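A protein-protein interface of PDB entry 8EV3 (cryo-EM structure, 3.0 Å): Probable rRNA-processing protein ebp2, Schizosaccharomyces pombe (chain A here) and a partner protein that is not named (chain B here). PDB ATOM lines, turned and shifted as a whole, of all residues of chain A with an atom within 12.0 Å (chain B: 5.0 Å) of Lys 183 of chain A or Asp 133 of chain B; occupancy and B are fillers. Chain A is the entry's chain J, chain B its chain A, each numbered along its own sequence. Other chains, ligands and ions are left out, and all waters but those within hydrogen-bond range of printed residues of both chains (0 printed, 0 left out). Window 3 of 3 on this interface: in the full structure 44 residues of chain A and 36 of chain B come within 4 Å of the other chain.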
ATOM      1  N   LEU A 175      11.145  13.172 -14.103  1.00  0.00           N
ATOM      2  CA  LEU A 175      10.079  12.170 -14.116  1.00  0.00           C
ATOM      3  C   LEU A 175      10.341  11.106 -13.048  1.00  0.00           C
ATOM      4  O   LEU A 175      10.487   9.915 -13.325  1.00  0.00           O
ATOM      5  CB  LEU A 175       9.953  11.551 -15.502  1.00  0.00           C
ATOM      6  N   LYS A 176      10.398  11.565 -11.799  1.00  0.00           N
ATOM      7  CA  LYS A 176      10.685  10.716 -10.643  1.00  0.00           C
ATOM      8  C   LYS A 176       9.571  10.920  -9.623  1.00  0.00           C
ATOM      9  O   LYS A 176       9.662  11.797  -8.758  1.00  0.00           O
ATOM     10  CB  LYS A 176      12.054  11.035 -10.050  1.00  0.00           C
ATOM     11  N   SER A 177       8.520  10.113  -9.727  1.00  0.00           N
ATOM     12  CA  SER A 177       7.459  10.146  -8.735  1.00  0.00           C
ATOM     13  C   SER A 177       7.953   9.559  -7.419  1.00  0.00           C
ATOM     14  O   SER A 177       8.947   8.829  -7.374  1.00  0.00           O
ATOM     15  CB  SER A 177       6.237   9.374  -9.232  1.00  0.00           C
ATOM     16  N   ASP A 178       7.251   9.898  -6.335  1.00  0.00           N
ATOM     17  CA  ASP A 178       7.637   9.391  -5.021  1.00  0.00           C
ATOM     18  C   ASP A 178       7.573   7.870  -4.978  1.00  0.00           C
ATOM     19  O   ASP A 178       8.487   7.217  -4.462  1.00  0.00           O
ATOM     20  CB  ASP A 178       6.743   9.998  -3.940  1.00  0.00           C
ATOM     21  N   ASP A 179       6.498   7.288  -5.515  1.00  0.00           N
ATOM     22  CA  ASP A 179       6.418   5.834  -5.607  1.00  0.00           C
ATOM     23  C   ASP A 179       7.434   5.288  -6.600  1.00  0.00           C
ATOM     24  O   ASP A 179       8.058   4.249  -6.352  1.00  0.00           O
ATOM     25  CB  ASP A 179       5.002   5.409  -5.997  1.00  0.00           C
ATOM     26  N   HIS A 180       7.611   5.970  -7.735  1.00  0.00           N
ATOM     27  CA  HIS A 180       8.558   5.505  -8.744  1.00  0.00           C
ATOM     28  C   HIS A 180       9.989   5.542  -8.223  1.00  0.00           C
ATOM     29  O   HIS A 180      10.764   4.605  -8.456  1.00  0.00           O
ATOM     30  CB  HIS A 180       8.427   6.346 -10.014  1.00  0.00           C
ATOM     31  N   MET A 181      10.363   6.616  -7.525  1.00  0.00           N
ATOM     32  CA  MET A 181      11.704   6.695  -6.954  1.00  0.00           C
ATOM     33  C   MET A 181      11.909   5.628  -5.886  1.00  0.00           C
ATOM     34  O   MET A 181      12.977   5.007  -5.813  1.00  0.00           O
ATOM     35  CB  MET A 181      11.952   8.089  -6.378  1.00  0.00           C
ATOM     36  N   GLU A 182      10.897   5.406  -5.043  1.00  0.00           N
ATOM     37  CA  GLU A 182      10.987   4.348  -4.042  1.00  0.00           C
ATOM     38  C   GLU A 182      11.061   2.975  -4.698  1.00  0.00           C
ATOM     39  O   GLU A 182      11.820   2.105  -4.253  1.00  0.00           O
ATOM     40  CB  GLU A 182       9.794   4.425  -3.089  1.00  0.00           C
ATOM     41  N   LYS A 183      10.276   2.761  -5.757  1.00  0.00           N
ATOM     42  CA  LYS A 183      10.335   1.494  -6.479  1.00  0.00           C
ATOM     43  C   LYS A 183      11.688   1.308  -7.154  1.00  0.00           C
ATOM     44  O   LYS A 183      12.209   0.188  -7.222  1.00  0.00           O
ATOM     45  CB  LYS A 183       9.207   1.422  -7.508  1.00  0.00           C
ATOM     46  N   VAL A 184      12.268   2.395  -7.669  1.00  0.00           N
ATOM     47  CA  VAL A 184      13.582   2.313  -8.303  1.00  0.00           C
ATOM     48  C   VAL A 184      14.636   1.887  -7.291  1.00  0.00           C
ATOM     49  O   VAL A 184      15.491   1.040  -7.579  1.00  0.00           O
ATOM     50  CB  VAL A 184      13.943   3.657  -8.962  1.00  0.00           C
ATOM     51  N   ARG A 185      14.594   2.464  -6.094  1.00  0.00           N
ATOM     52  CA  ARG A 185      15.550   2.128  -5.047  1.00  0.00           C
ATOM     53  C   ARG A 185      15.053   0.954  -4.209  1.00  0.00           C
ATOM     54  O   ARG A 185      14.093   0.278  -4.579  1.00  0.00           O
ATOM     55  CB  ARG A 185      15.811   3.341  -4.152  1.00  0.00           C
ATOM     56  N   HIS B  59      -3.595   2.907 -16.132  1.00  0.00           N
ATOM     57  CA  HIS B  59      -2.275   3.130 -15.553  1.00  0.00           C
ATOM     58  C   HIS B  59      -1.312   3.687 -16.593  1.00  0.00           C
ATOM     59  O   HIS B  59      -0.658   4.710 -16.367  1.00  0.00           O
ATOM     60  CB  HIS B  59      -1.734   1.830 -14.959  1.00  0.00           C
ATOM     61  CG  HIS B  59      -1.198   1.977 -13.570  1.00  0.00           C
ATOM     62  ND1 HIS B  59      -0.217   2.888 -13.243  1.00  0.00           N
ATOM     63  CD2 HIS B  59      -1.508   1.329 -12.422  1.00  0.00           C
ATOM     64  CE1 HIS B  59       0.054   2.794 -11.953  1.00  0.00           C
ATOM     65  NE2 HIS B  59      -0.715   1.856 -11.432  1.00  0.00           N
ATOM     66  N   THR B 131       4.202  -1.016 -16.163  1.00  0.00           N
ATOM     67  CA  THR B 131       3.714   0.218 -15.567  1.00  0.00           C
ATOM     68  C   THR B 131       4.828   0.954 -14.824  1.00  0.00           C
ATOM     69  O   THR B 131       5.940   0.449 -14.643  1.00  0.00           O
ATOM     70  CB  THR B 131       2.552  -0.064 -14.615  1.00  0.00           C
ATOM     71  OG1 THR B 131       2.848  -1.219 -13.818  1.00  0.00           O
ATOM     72  CG2 THR B 131       1.267  -0.298 -15.392  1.00  0.00           C
ATOM     73  N   MET B 132       4.507   2.177 -14.393  1.00  0.00           N
ATOM     74  CA  MET B 132       5.457   2.975 -13.625  1.00  0.00           C
ATOM     75  C   MET B 132       5.662   2.417 -12.223  1.00  0.00           C
ATOM     76  O   MET B 132       6.776   2.475 -11.690  1.00  0.00           O
ATOM     77  CB  MET B 132       4.978   4.426 -13.537  1.00  0.00           C
ATOM     78  CG  MET B 132       5.288   5.351 -14.729  1.00  0.00           C
ATOM     79  SD  MET B 132       6.807   5.110 -15.681  1.00  0.00           S
ATOM     80  CE  MET B 132       6.371   3.750 -16.765  1.00  0.00           C
ATOM     81  N   ASP B 133       4.604   1.877 -11.614  1.00  0.00           N
ATOM     82  CA  ASP B 133       4.666   1.429 -10.227  1.00  0.00           C
ATOM     83  C   ASP B 133       5.583   0.227 -10.034  1.00  0.00           C
ATOM     84  O   ASP B 133       5.993  -0.045  -8.900  1.00  0.00           O
ATOM     85  CB  ASP B 133       3.259   1.099  -9.726  1.00  0.00           C
ATOM     86  CG  ASP B 133       3.205   0.892  -8.225  1.00  0.00           C
ATOM     87  OD1 ASP B 133       4.025   1.501  -7.509  1.00  0.00           O
ATOM     88  OD2 ASP B 133       2.342   0.117  -7.761  1.00  0.00           O
ATOM     89  N   GLU B 134       5.910  -0.496 -11.102  1.00  0.00           N
ATOM     90  CA  GLU B 134       6.768  -1.665 -10.970  1.00  0.00           C
ATOM     91  C   GLU B 134       8.165  -1.261 -10.511  1.00  0.00           C
ATOM     92  O   GLU B 134       8.689  -0.209 -10.887  1.00  0.00           O
ATOM     93  CB  GLU B 134       6.845  -2.422 -12.297  1.00  0.00           C
ATOM     94  CG  GLU B 134       5.498  -2.915 -12.800  1.00  0.00           C
ATOM     95  CD  GLU B 134       5.618  -3.785 -14.036  1.00  0.00           C
ATOM     96  OE1 GLU B 134       6.725  -4.302 -14.294  1.00  0.00           O
ATOM     97  OE2 GLU B 134       4.606  -3.952 -14.749  1.00  0.00           O
ATOM     98  N   LEU B 135       8.768  -2.113  -9.679  1.00  0.00           N
ATOM     99  CA  LEU B 135      10.090  -1.824  -9.136  1.00  0.00           C
ATOM    100  C   LEU B 135      11.178  -1.845 -10.201  1.00  0.00           C
ATOM    101  O   LEU B 135      12.252  -1.275  -9.980  1.00  0.00           O
ATOM    102  CB  LEU B 135      10.429  -2.815  -8.022  1.00  0.00           C
ATOM    103  CG  LEU B 135       9.264  -3.240  -7.123  1.00  0.00           C
ATOM    104  CD1 LEU B 135       9.684  -4.368  -6.195  1.00  0.00           C
ATOM    105  CD2 LEU B 135       8.739  -2.055  -6.326  1.00  0.00           C
ATOM    106  N   MET B 137      11.184  -0.178 -12.783  1.00  0.00           N
ATOM    107  CA  MET B 137      11.330   1.206 -13.213  1.00  0.00           C
ATOM    108  C   MET B 137      12.593   1.811 -12.612  1.00  0.00           C
ATOM    109  O   MET B 137      12.687   1.981 -11.393  1.00  0.00           O
ATOM    110  CB  MET B 137      10.092   2.014 -12.811  1.00  0.00           C
ATOM    111  CG  MET B 137      10.170   3.518 -13.053  1.00  0.00           C
ATOM    112  SD  MET B 137      11.197   4.013 -14.447  1.00  0.00           S
ATOM    113  CE  MET B 137      11.536   5.719 -14.025  1.00  0.00           C
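The side-chain carboxylate of Glu 134 of chain B sits at hydrogen-bond distance from the backbone NH of Thr 131 of chain B (3.3 Å).
Asp 179 of chain A touches none of the printed residues of chain B. Met 181 of chain A touches none of the printed residues of chain B. Lys 183 of chain A touches just these residues of chain B: Asp 133, Glu 134 and Leu 135. Printed residues of chain B within 4 Å of Val 184 of chain A: Met 137 (3.2 Å). No residue of chain A comes within 4 Å of Thr 131 of chain B. No residue of chain A comes within 4 Å of Met 132 of chain B. Of chain A, only Lys 183 comes within 4 Å of Asp 133 of chain B. Glu 134 of chain B touches one residue of chain A. Leu 135 of chain B touches just one residue of chain A: Lys 183 (3.1 Å). Of the printed residues of chain A, Met 137 of chain B touches Val 184 (3.2 Å). The nearest residue of chain B that does not touch Lys 183 of chain A is Met 137 of chain B (4.4 Å). The nearest residue of chain A that does not touch Asp 133 of chain B is Asp 179 of chain A (4.3 Å).
The backbone carbonyl oxygen of Leu 135 of chain B lies close to the backbone carbonyl oxygen of Lys 183 of chain A, 3.1 Å away.
Hydrophobic or aromatic side chains of chain B within 4 Å of the printed part of chain A: Leu 135. Hydrophobic or aromatic side chains of chain A within 4 Å of the printed part of chain B: Val 184. Among the printed residues, no Asp or Glu carboxylate lies within 4 Å of a Lys or Arg side-chain nitrogen of the other chain.
Asp 133 of chain B touches Lys 183 of chain A. Lys 183 of chain A touches Glu 134 of chain B. Met 137 of chain B touches Val 184 of chain A.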
